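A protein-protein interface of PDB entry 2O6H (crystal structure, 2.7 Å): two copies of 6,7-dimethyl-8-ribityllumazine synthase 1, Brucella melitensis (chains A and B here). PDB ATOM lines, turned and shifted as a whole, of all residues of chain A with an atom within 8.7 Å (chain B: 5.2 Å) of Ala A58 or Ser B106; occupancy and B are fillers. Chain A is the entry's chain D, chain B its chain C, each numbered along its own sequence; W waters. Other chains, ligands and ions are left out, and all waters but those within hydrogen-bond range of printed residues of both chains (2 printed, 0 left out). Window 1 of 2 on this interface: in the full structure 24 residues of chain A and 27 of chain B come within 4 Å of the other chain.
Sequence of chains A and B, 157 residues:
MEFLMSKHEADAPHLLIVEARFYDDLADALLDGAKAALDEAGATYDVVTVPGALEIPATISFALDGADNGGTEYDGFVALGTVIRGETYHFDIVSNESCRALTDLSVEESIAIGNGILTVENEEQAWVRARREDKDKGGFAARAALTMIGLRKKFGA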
ATOM      1  N   LEU A  16     -16.780 -23.587  23.071  1.00  0.00           N
ATOM      2  CA  LEU A  16     -17.491 -22.560  23.806  1.00  0.00           C
ATOM      3  C   LEU A  16     -17.976 -21.595  22.732  1.00  0.00           C
ATOM      4  O   LEU A  16     -17.167 -20.956  22.059  1.00  0.00           O
ATOM      5  CB  LEU A  16     -16.573 -21.797  24.753  1.00  0.00           C
ATOM      6  CG  LEU A  16     -17.305 -20.578  25.335  1.00  0.00           C
ATOM      7  CD1 LEU A  16     -18.200 -20.994  26.504  1.00  0.00           C
ATOM      8  CD2 LEU A  16     -16.293 -19.550  25.778  1.00  0.00           C
ATOM      9  N   VAL A  18     -19.401 -18.244  21.912  1.00  0.00           N
ATOM     10  CA  VAL A  18     -19.633 -16.932  22.497  1.00  0.00           C
ATOM     11  C   VAL A  18     -20.420 -16.082  21.504  1.00  0.00           C
ATOM     12  O   VAL A  18     -19.863 -15.591  20.523  1.00  0.00           O
ATOM     13  CB  VAL A  18     -18.320 -16.228  22.841  1.00  0.00           C
ATOM     14  CG1 VAL A  18     -18.595 -14.816  23.284  1.00  0.00           C
ATOM     15  CG2 VAL A  18     -17.618 -16.975  23.941  1.00  0.00           C
ATOM     16  N   VAL A  48     -22.435 -19.196  25.626  1.00  0.00           N
ATOM     17  CA  VAL A  48     -22.530 -18.053  26.539  1.00  0.00           C
ATOM     18  C   VAL A  48     -23.009 -16.824  25.744  1.00  0.00           C
ATOM     19  O   VAL A  48     -22.661 -16.651  24.576  1.00  0.00           O
ATOM     20  CB  VAL A  48     -21.178 -17.773  27.243  1.00  0.00           C
ATOM     21  CG1 VAL A  48     -20.109 -17.423  26.230  1.00  0.00           C
ATOM     22  CG2 VAL A  48     -21.336 -16.662  28.231  1.00  0.00           C
ATOM     23  N   VAL A  50     -23.518 -12.592  25.351  1.00  0.00           N
ATOM     24  CA  VAL A  50     -23.037 -11.269  25.715  1.00  0.00           C
ATOM     25  C   VAL A  50     -23.871 -10.247  24.941  1.00  0.00           C
ATOM     26  O   VAL A  50     -24.402 -10.556  23.881  1.00  0.00           O
ATOM     27  CB  VAL A  50     -21.545 -11.102  25.349  1.00  0.00           C
ATOM     28  CG1 VAL A  50     -20.711 -12.096  26.132  1.00  0.00           C
ATOM     29  CG2 VAL A  50     -21.344 -11.303  23.839  1.00  0.00           C
ATOM     30  N   GLY A  52     -23.074  -7.194  23.237  1.00  0.00           N
ATOM     31  CA  GLY A  52     -22.609  -6.779  21.930  1.00  0.00           C
ATOM     32  C   GLY A  52     -21.300  -7.434  21.555  1.00  0.00           C
ATOM     33  O   GLY A  52     -20.572  -7.928  22.413  1.00  0.00           O
ATOM     34  N   ALA A  53     -20.999  -7.424  20.260  1.00  0.00           N
ATOM     35  CA  ALA A  53     -19.778  -8.018  19.737  1.00  0.00           C
ATOM     36  C   ALA A  53     -18.540  -7.512  20.465  1.00  0.00           C
ATOM     37  O   ALA A  53     -17.521  -8.205  20.509  1.00  0.00           O
ATOM     38  CB  ALA A  53     -19.656  -7.724  18.247  1.00  0.00           C
ATOM     39  N   LEU A  54     -18.612  -6.310  21.029  1.00  0.00           N
ATOM     40  CA  LEU A  54     -17.458  -5.774  21.735  1.00  0.00           C
ATOM     41  C   LEU A  54     -17.023  -6.616  22.929  1.00  0.00           C
ATOM     42  O   LEU A  54     -15.838  -6.637  23.257  1.00  0.00           O
ATOM     43  CB  LEU A  54     -17.704  -4.345  22.219  1.00  0.00           C
ATOM     44  CG  LEU A  54     -17.667  -3.174  21.241  1.00  0.00           C
ATOM     45  CD1 LEU A  54     -17.578  -1.901  22.068  1.00  0.00           C
ATOM     46  CD2 LEU A  54     -16.476  -3.271  20.299  1.00  0.00           C
ATOM     47  N   GLU A  55     -17.947  -7.298  23.604  1.00  0.00           N
ATOM     48  CA  GLU A  55     -17.501  -8.103  24.740  1.00  0.00           C
ATOM     49  C   GLU A  55     -17.136  -9.553  24.420  1.00  0.00           C
ATOM     50  O   GLU A  55     -16.859 -10.331  25.330  1.00  0.00           O
ATOM     51  CB  GLU A  55     -18.486  -8.056  25.934  1.00  0.00           C
ATOM     52  CG  GLU A  55     -19.920  -7.675  25.664  1.00  0.00           C
ATOM     53  CD  GLU A  55     -20.118  -6.182  25.448  1.00  0.00           C
ATOM     54  OE1 GLU A  55     -19.433  -5.371  26.105  1.00  0.00           O
ATOM     55  OE2 GLU A  55     -20.982  -5.822  24.625  1.00  0.00           O
ATOM     56  N   ILE A  56     -17.100  -9.909  23.139  1.00  0.00           N
ATOM     57  CA  ILE A  56     -16.734 -11.268  22.746  1.00  0.00           C
ATOM     58  C   ILE A  56     -15.313 -11.640  23.221  1.00  0.00           C
ATOM     59  O   ILE A  56     -15.122 -12.624  23.941  1.00  0.00           O
ATOM     60  CB  ILE A  56     -16.832 -11.446  21.216  1.00  0.00           C
ATOM     61  CG1 ILE A  56     -18.298 -11.512  20.802  1.00  0.00           C
ATOM     62  CG2 ILE A  56     -16.107 -12.709  20.782  1.00  0.00           C
ATOM     63  CD1 ILE A  56     -18.511 -11.636  19.299  1.00  0.00           C
ATOM     64  N   PRO A  57     -14.296 -10.862  22.822  1.00  0.00           N
ATOM     65  CA  PRO A  57     -12.960 -11.229  23.286  1.00  0.00           C
ATOM     66  C   PRO A  57     -12.823 -11.361  24.812  1.00  0.00           C
ATOM     67  O   PRO A  57     -12.288 -12.354  25.301  1.00  0.00           O
ATOM     68  CB  PRO A  57     -12.072 -10.118  22.699  1.00  0.00           C
ATOM     69  CG  PRO A  57     -13.010  -8.967  22.532  1.00  0.00           C
ATOM     70  CD  PRO A  57     -14.241  -9.643  21.996  1.00  0.00           C
ATOM     71  N   ALA A  58     -13.308 -10.372  25.560  1.00  0.00           N
ATOM     72  CA  ALA A  58     -13.204 -10.405  27.022  1.00  0.00           C
ATOM     73  C   ALA A  58     -13.764 -11.696  27.585  1.00  0.00           C
ATOM     74  O   ALA A  58     -13.198 -12.262  28.510  1.00  0.00           O
ATOM     75  CB  ALA A  58     -13.925  -9.213  27.644  1.00  0.00           C
ATOM     76  N   THR A  59     -14.875 -12.160  27.026  1.00  0.00           N
ATOM     77  CA  THR A  59     -15.484 -13.396  27.490  1.00  0.00           C
ATOM     78  C   THR A  59     -14.561 -14.600  27.245  1.00  0.00           C
ATOM     79  O   THR A  59     -14.431 -15.468  28.107  1.00  0.00           O
ATOM     80  CB  THR A  59     -16.852 -13.625  26.824  1.00  0.00           C
ATOM     81  OG1 THR A  59     -17.708 -12.507  27.102  1.00  0.00           O
ATOM     82  CG2 THR A  59     -17.501 -14.892  27.370  1.00  0.00           C
ATOM     83  N   ILE A  60     -13.918 -14.663  26.085  1.00  0.00           N
ATOM     84  CA  ILE A  60     -12.998 -15.762  25.834  1.00  0.00           C
ATOM     85  C   ILE A  60     -11.847 -15.600  26.838  1.00  0.00           C
ATOM     86  O   ILE A  60     -11.243 -16.573  27.297  1.00  0.00           O
ATOM     87  CB  ILE A  60     -12.455 -15.723  24.380  1.00  0.00           C
ATOM     88  CG1 ILE A  60     -13.576 -16.090  23.403  1.00  0.00           C
ATOM     89  CG2 ILE A  60     -11.275 -16.685  24.219  1.00  0.00           C
ATOM     90  CD1 ILE A  60     -13.167 -16.021  21.955  1.00  0.00           C
ATOM     91  N   SER A  61     -11.560 -14.356  27.193  1.00  0.00           N
ATOM     92  CA  SER A  61     -10.506 -14.077  28.154  1.00  0.00           C
ATOM     93  C   SER A  61     -10.908 -14.634  29.516  1.00  0.00           C
ATOM     94  O   SER A  61     -10.082 -15.208  30.207  1.00  0.00           O
ATOM     95  CB  SER A  61     -10.258 -12.569  28.247  1.00  0.00           C
ATOM     96  OG  SER A  61      -9.219 -12.258  29.158  1.00  0.00           O
ATOM     97  N   PHE A  62     -12.171 -14.459  29.901  1.00  0.00           N
ATOM     98  CA  PHE A  62     -12.671 -14.969  31.183  1.00  0.00           C
ATOM     99  C   PHE A  62     -12.592 -16.493  31.177  1.00  0.00           C
ATOM    100  O   PHE A  62     -12.235 -17.117  32.181  1.00  0.00           O
ATOM    101  CB  PHE A  62     -14.136 -14.573  31.408  1.00  0.00           C
ATOM    102  CG  PHE A  62     -14.363 -13.097  31.544  1.00  0.00           C
ATOM    103  CD1 PHE A  62     -15.637 -12.568  31.354  1.00  0.00           C
ATOM    104  CD2 PHE A  62     -13.321 -12.237  31.881  1.00  0.00           C
ATOM    105  CE1 PHE A  62     -15.875 -11.201  31.497  1.00  0.00           C
ATOM    106  CE2 PHE A  62     -13.548 -10.870  32.028  1.00  0.00           C
ATOM    107  CZ  PHE A  62     -14.829 -10.348  31.836  1.00  0.00           C
ATOM    108  N   ALA A  63     -12.956 -17.086  30.044  1.00  0.00           N
ATOM    109  CA  ALA A  63     -12.922 -18.532  29.899  1.00  0.00           C
ATOM    110  C   ALA A  63     -11.480 -19.040  30.063  1.00  0.00           C
ATOM    111  O   ALA A  63     -11.233 -20.076  30.694  1.00  0.00           O
ATOM    112  CB  ALA A  63     -13.473 -18.925  28.532  1.00  0.00           C
ATOM    113  N   LEU A  64     -10.535 -18.294  29.495  1.00  0.00           N
ATOM    114  CA  LEU A  64      -9.123 -18.652  29.566  1.00  0.00           C
ATOM    115  C   LEU A  64      -8.575 -18.586  30.986  1.00  0.00           C
ATOM    116  O   LEU A  64      -7.723 -19.388  31.363  1.00  0.00           O
ATOM    117  CB  LEU A  64      -8.293 -17.741  28.650  1.00  0.00           C
ATOM    118  CG  LEU A  64      -8.528 -17.894  27.148  1.00  0.00           C
ATOM    119  CD1 LEU A  64      -7.416 -17.204  26.427  1.00  0.00           C
ATOM    120  CD2 LEU A  64      -8.563 -19.356  26.748  1.00  0.00           C
ATOM    121  N   ASP A  65      -9.059 -17.622  31.762  1.00  0.00           N
ATOM    122  CA  ASP A  65      -8.640 -17.459  33.148  1.00  0.00           C
ATOM    123  C   ASP A  65      -9.275 -18.559  33.982  1.00  0.00           C
ATOM    124  O   ASP A  65      -8.612 -19.202  34.796  1.00  0.00           O
ATOM    125  CB  ASP A  65      -9.071 -16.094  33.668  1.00  0.00           C
ATOM    126  CG  ASP A  65      -8.051 -15.010  33.380  1.00  0.00           C
ATOM    127  OD1 ASP A  65      -7.405 -15.050  32.313  1.00  0.00           O
ATOM    128  OD2 ASP A  65      -7.904 -14.104  34.223  1.00  0.00           O
ATOM    129  N   GLU A  97     -12.926  -3.211  16.498  1.00  0.00           N
ATOM    130  CA  GLU A  97     -12.417  -3.718  17.758  1.00  0.00           C
ATOM    131  C   GLU A  97     -12.725  -5.171  18.099  1.00  0.00           C
ATOM    132  O   GLU A  97     -11.923  -5.835  18.750  1.00  0.00           O
ATOM    133  CB  GLU A  97     -12.867  -2.802  18.892  1.00  0.00           C
ATOM    134  CG  GLU A  97     -12.592  -1.347  18.589  1.00  0.00           C
ATOM    135  CD  GLU A  97     -11.224  -1.125  17.962  1.00  0.00           C
ATOM    136  OE1 GLU A  97     -11.054  -0.097  17.264  1.00  0.00           O
ATOM    137  OE2 GLU A  97     -10.317  -1.965  18.168  1.00  0.00           O
ATOM    138  N   SER A  98     -13.866  -5.678  17.658  1.00  0.00           N
ATOM    139  CA  SER A  98     -14.206  -7.053  17.968  1.00  0.00           C
ATOM    140  C   SER A  98     -13.356  -8.036  17.166  1.00  0.00           C
ATOM    141  O   SER A  98     -12.912  -9.062  17.690  1.00  0.00           O
ATOM    142  CB  SER A  98     -15.701  -7.304  17.722  1.00  0.00           C
ATOM    143  OG  SER A  98     -16.055  -7.046  16.378  1.00  0.00           O
ATOM    144  N   ALA A 101      -9.421  -7.612  18.331  1.00  0.00           N
ATOM    145  CA  ALA A 101      -9.101  -8.266  19.600  1.00  0.00           C
ATOM    146  C   ALA A 101      -9.081  -9.789  19.449  1.00  0.00           C
ATOM    147  O   ALA A 101      -8.225 -10.453  20.028  1.00  0.00           O
ATOM    148  CB  ALA A 101     -10.094  -7.851  20.679  1.00  0.00           C
ATOM    149  N   LEU A 102     -10.015 -10.336  18.668  1.00  0.00           N
ATOM    150  CA  LEU A 102     -10.085 -11.783  18.440  1.00  0.00           C
ATOM    151  C   LEU A 102      -8.833 -12.313  17.764  1.00  0.00           C
ATOM    152  O   LEU A 102      -8.123 -13.152  18.317  1.00  0.00           O
ATOM    153  CB  LEU A 102     -11.272 -12.151  17.556  1.00  0.00           C
ATOM    154  CG  LEU A 102     -12.570 -12.630  18.186  1.00  0.00           C
ATOM    155  CD1 LEU A 102     -13.365 -13.345  17.104  1.00  0.00           C
ATOM    156  CD2 LEU A 102     -12.309 -13.581  19.337  1.00  0.00           C
ATOM    157  N   LEU A 105      -6.193 -12.419  20.104  1.00  0.00           N
ATOM    158  CA  LEU A 105      -6.368 -13.452  21.106  1.00  0.00           C
ATOM    159  C   LEU A 105      -5.966 -14.832  20.558  1.00  0.00           C
ATOM    160  O   LEU A 105      -5.249 -15.580  21.219  1.00  0.00           O
ATOM    161  CB  LEU A 105      -7.830 -13.439  21.585  1.00  0.00           C
ATOM    162  CG  LEU A 105      -8.155 -13.970  22.978  1.00  0.00           C
ATOM    163  CD1 LEU A 105      -7.384 -13.175  24.009  1.00  0.00           C
ATOM    164  CD2 LEU A 105      -9.654 -13.871  23.229  1.00  0.00           C
ATOM    165  N   LEU B 102      -9.593   0.679  25.093  1.00  0.00           N
ATOM    166  CA  LEU B 102     -10.557   0.171  26.065  1.00  0.00           C
ATOM    167  C   LEU B 102     -10.841  -1.311  25.827  1.00  0.00           C
ATOM    168  O   LEU B 102     -11.067  -2.062  26.770  1.00  0.00           O
ATOM    169  CB  LEU B 102     -11.855   0.965  25.972  1.00  0.00           C
ATOM    170  CG  LEU B 102     -12.627   1.321  27.243  1.00  0.00           C
ATOM    171  CD1 LEU B 102     -14.034   1.769  26.846  1.00  0.00           C
ATOM    172  CD2 LEU B 102     -12.712   0.137  28.170  1.00  0.00           C
ATOM    173  N   THR B 103     -10.823  -1.737  24.570  1.00  0.00           N
ATOM    174  CA  THR B 103     -11.078  -3.136  24.263  1.00  0.00           C
ATOM    175  C   THR B 103      -9.915  -4.004  24.726  1.00  0.00           C
ATOM    176  O   THR B 103     -10.124  -4.986  25.436  1.00  0.00           O
ATOM    177  CB  THR B 103     -11.289  -3.352  22.756  1.00  0.00           C
ATOM    178  OG1 THR B 103     -12.178  -2.349  22.254  1.00  0.00           O
ATOM    179  CG2 THR B 103     -11.900  -4.725  22.497  1.00  0.00           C
ATOM    180  N   ASP B 104      -8.692  -3.647  24.334  1.00  0.00           N
ATOM    181  CA  ASP B 104      -7.522  -4.423  24.749  1.00  0.00           C
ATOM    182  C   ASP B 104      -7.555  -4.648  26.256  1.00  0.00           C
ATOM    183  O   ASP B 104      -7.422  -5.776  26.737  1.00  0.00           O
ATOM    184  CB  ASP B 104      -6.207  -3.703  24.445  1.00  0.00           C
ATOM    185  CG  ASP B 104      -5.955  -3.519  22.979  1.00  0.00           C
ATOM    186  OD1 ASP B 104      -6.376  -4.378  22.175  1.00  0.00           O
ATOM    187  OD2 ASP B 104      -5.303  -2.508  22.636  1.00  0.00           O
ATOM    188  N   LEU B 105      -7.715  -3.552  26.991  1.00  0.00           N
ATOM    189  CA  LEU B 105      -7.740  -3.596  28.436  1.00  0.00           C
ATOM    190  C   LEU B 105      -8.671  -4.686  28.974  1.00  0.00           C
ATOM    191  O   LEU B 105      -8.238  -5.532  29.763  1.00  0.00           O
ATOM    192  CB  LEU B 105      -8.130  -2.221  28.980  1.00  0.00           C
ATOM    193  CG  LEU B 105      -7.780  -1.873  30.432  1.00  0.00           C
ATOM    194  CD1 LEU B 105      -6.326  -2.206  30.752  1.00  0.00           C
ATOM    195  CD2 LEU B 105      -8.042  -0.393  30.638  1.00  0.00           C
ATOM    196  N   SER B 106      -9.930  -4.694  28.539  1.00  0.00           N
ATOM    197  CA  SER B 106     -10.885  -5.700  29.013  1.00  0.00           C
ATOM    198  C   SER B 106     -10.325  -7.109  28.874  1.00  0.00           C
ATOM    199  O   SER B 106     -10.578  -7.975  29.711  1.00  0.00           O
ATOM    200  CB  SER B 106     -12.211  -5.610  28.242  1.00  0.00           C
ATOM    201  OG  SER B 106     -12.091  -6.088  26.914  1.00  0.00           O
ATOM    202  N   VAL B 107      -9.558  -7.331  27.813  1.00  0.00           N
ATOM    203  CA  VAL B 107      -8.957  -8.636  27.552  1.00  0.00           C
ATOM    204  C   VAL B 107      -7.654  -8.898  28.315  1.00  0.00           C
ATOM    205  O   VAL B 107      -7.483  -9.954  28.921  1.00  0.00           O
ATOM    206  CB  VAL B 107      -8.677  -8.804  26.058  1.00  0.00           C
ATOM    207  CG1 VAL B 107      -7.740  -9.959  25.838  1.00  0.00           C
ATOM    208  CG2 VAL B 107      -9.979  -9.035  25.319  1.00  0.00           C
ATOM    209  N   GLU B 108      -6.748  -7.929  28.281  1.00  0.00           N
ATOM    210  CA  GLU B 108      -5.455  -8.061  28.934  1.00  0.00           C
ATOM    211  C   GLU B 108      -5.528  -8.165  30.453  1.00  0.00           C
ATOM    212  O   GLU B 108      -4.670  -8.796  31.071  1.00  0.00           O
ATOM    213  CB  GLU B 108      -4.554  -6.885  28.534  1.00  0.00           C
ATOM    214  CG  GLU B 108      -3.101  -6.971  29.010  1.00  0.00           C
ATOM    215  CD  GLU B 108      -2.199  -5.931  28.337  1.00  0.00           C
ATOM    216  OE1 GLU B 108      -1.022  -5.808  28.744  1.00  0.00           O
ATOM    217  OE2 GLU B 108      -2.662  -5.239  27.393  1.00  0.00           O
ATOM    218  N   GLU B 109      -6.541  -7.559  31.060  1.00  0.00           N
ATOM    219  CA  GLU B 109      -6.666  -7.603  32.514  1.00  0.00           C
ATOM    220  C   GLU B 109      -7.860  -8.434  32.947  1.00  0.00           C
ATOM    221  O   GLU B 109      -8.149  -8.533  34.135  1.00  0.00           O
ATOM    222  CB  GLU B 109      -6.834  -6.194  33.065  1.00  0.00           C
ATOM    223  CG  GLU B 109      -5.741  -5.228  32.679  1.00  0.00           C
ATOM    224  CD  GLU B 109      -4.490  -5.431  33.491  1.00  0.00           C
ATOM    225  OE1 GLU B 109      -4.587  -5.394  34.738  1.00  0.00           O
ATOM    226  OE2 GLU B 109      -3.415  -5.623  32.883  1.00  0.00           O
ATOM    227  N   SER B 110      -8.554  -9.020  31.975  1.00  0.00           N
ATOM    228  CA  SER B 110      -9.742  -9.829  32.244  1.00  0.00           C
ATOM    229  C   SER B 110     -10.779  -9.108  33.115  1.00  0.00           C
ATOM    230  O   SER B 110     -11.265  -9.658  34.102  1.00  0.00           O
ATOM    231  CB  SER B 110      -9.345 -11.157  32.904  1.00  0.00           C
ATOM    232  OG  SER B 110      -8.830 -12.075  31.954  1.00  0.00           O
ATOM    233  N   ILE B 111     -11.128  -7.881  32.738  1.00  0.00           N
ATOM    234  CA  ILE B 111     -12.109  -7.105  33.501  1.00  0.00           C
ATOM    235  C   ILE B 111     -13.413  -6.865  32.736  1.00  0.00           C
ATOM    236  O   ILE B 111     -13.444  -6.928  31.510  1.00  0.00           O
ATOM    237  CB  ILE B 111     -11.527  -5.735  33.929  1.00  0.00           C
ATOM    238  CG1 ILE B 111     -11.005  -4.991  32.696  1.00  0.00           C
ATOM    239  CG2 ILE B 111     -10.416  -5.941  34.955  1.00  0.00           C
ATOM    240  CD1 ILE B 111     -10.503  -3.592  32.993  1.00  0.00           C
ATOM    241  N   ILE B 113     -16.184  -4.480  31.361  1.00  0.00           N
ATOM    242  CA  ILE B 113     -16.337  -3.081  30.972  1.00  0.00           C
ATOM    243  C   ILE B 113     -17.540  -2.850  30.080  1.00  0.00           C
ATOM    244  O   ILE B 113     -17.752  -3.575  29.109  1.00  0.00           O
ATOM    245  CB  ILE B 113     -15.128  -2.583  30.175  1.00  0.00           C
ATOM    246  CG1 ILE B 113     -13.847  -2.751  30.995  1.00  0.00           C
ATOM    247  CG2 ILE B 113     -15.345  -1.134  29.781  1.00  0.00           C
ATOM    248  CD1 ILE B 113     -12.563  -2.327  30.258  1.00  0.00           C
ATOM    249  N   MET B 148     -21.366  -8.570  32.073  1.00  0.00           N
ATOM    250  CA  MET B 148     -19.997  -9.036  31.997  1.00  0.00           C
ATOM    251  C   MET B 148     -19.487  -9.427  33.363  1.00  0.00           C
ATOM    252  O   MET B 148     -18.723 -10.388  33.479  1.00  0.00           O
ATOM    253  CB  MET B 148     -19.075  -7.979  31.389  1.00  0.00           C
ATOM    254  CG  MET B 148     -19.139  -7.908  29.877  1.00  0.00           C
ATOM    255  SD  MET B 148     -19.208  -9.546  29.131  1.00  0.00           S
ATOM    256  CE  MET B 148     -17.477  -9.810  28.667  1.00  0.00           C
HETATM  257  O   HOH W   1      -5.765 -12.192  31.705  1.00  0.00           O
HETATM  258  O   HOH W   2     -17.086  -3.880  26.502  1.00  0.00           O
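The side-chain hydroxyl (OG) of Ser B110 is in hydrogen-bond range of the side-chain hydroxyl (OG) of Ser A61 (2.8 Å).
The side-chain carboxylate (OD2) of Asp A65 is in hydrogen-bond range of the side-chain hydroxyl (OG) of Ser B110, at 3.2 Å.
The backbone carbonyl oxygen (O) of Val B107 lies within hydrogen-bond range of the side-chain hydroxyl (OG) of Ser A61, 2.9 Å away.
O of Ser B106 is in hydrogen-bond range of N of Ile B111 (3.1 Å).
O of Thr B103 sits at hydrogen-bond distance from OG of Ser B106 (2.7 Å).
The backbone NH (N) of Gly A52 sits at hydrogen-bond distance from the side-chain carboxylate (OE2) of Glu A55.
O of Glu A55 lies within hydrogen-bond range of OG1 of Thr A59, 2.9 Å away.
Among the printed residues, merely in contact across the chains: Thr A59 with Met B148, Phe A62 with Ser B110, Glu A55 with Met B148, Glu A97 with Thr B103, Pro A57 with Val B107, Phe A62 with Met B148, Ala A58 with Val B107, Ala A58 with Ser B106, Phe A62 with Ile B111, Leu A105 with Val B107, Ala A58 with Met B148 and Glu A55 with Ile B113.
Ala A58 touches just these residues of chain B: Ser B106, Val B107 and Met B148.
Of the printed residues of chain B, Thr A59 touches Met B148.
Of the printed residues of chain B, Asp A65 touches Ser B110 (3.2 Å).
Of chain A, only Ala A58 comes within 4 Å of Ser B106.
Printed residues of chain A that touch a printed residue of chain B: Glu A55, Pro A57, Ala A58, Thr A59, Ser A61, Phe A62, Asp A65, Glu A97 and Leu A105.
Printed residues of chain B that touch a printed residue of chain A: Thr B103, Ser B106, Val B107, Ser B110, Ile B111, Ile B113 and Met B148.
Hydrophobic or aromatic side chains of chain B within 4 Å of the printed part of chain A: Val B107 and Met B148.
Among the printed residues, 15 pairs touch across the chains.
2 positions are printed for both chains.
Of the 15 pairs that touch across the chains among the printed residues, none has its exchanged pair printed and touching as well.
Water W2 lies within hydrogen-bond range of O of Ile B113 and OE1 of Glu A55.
Water W1 bridges OG of Ser B110 and OD1 of Asp A65.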
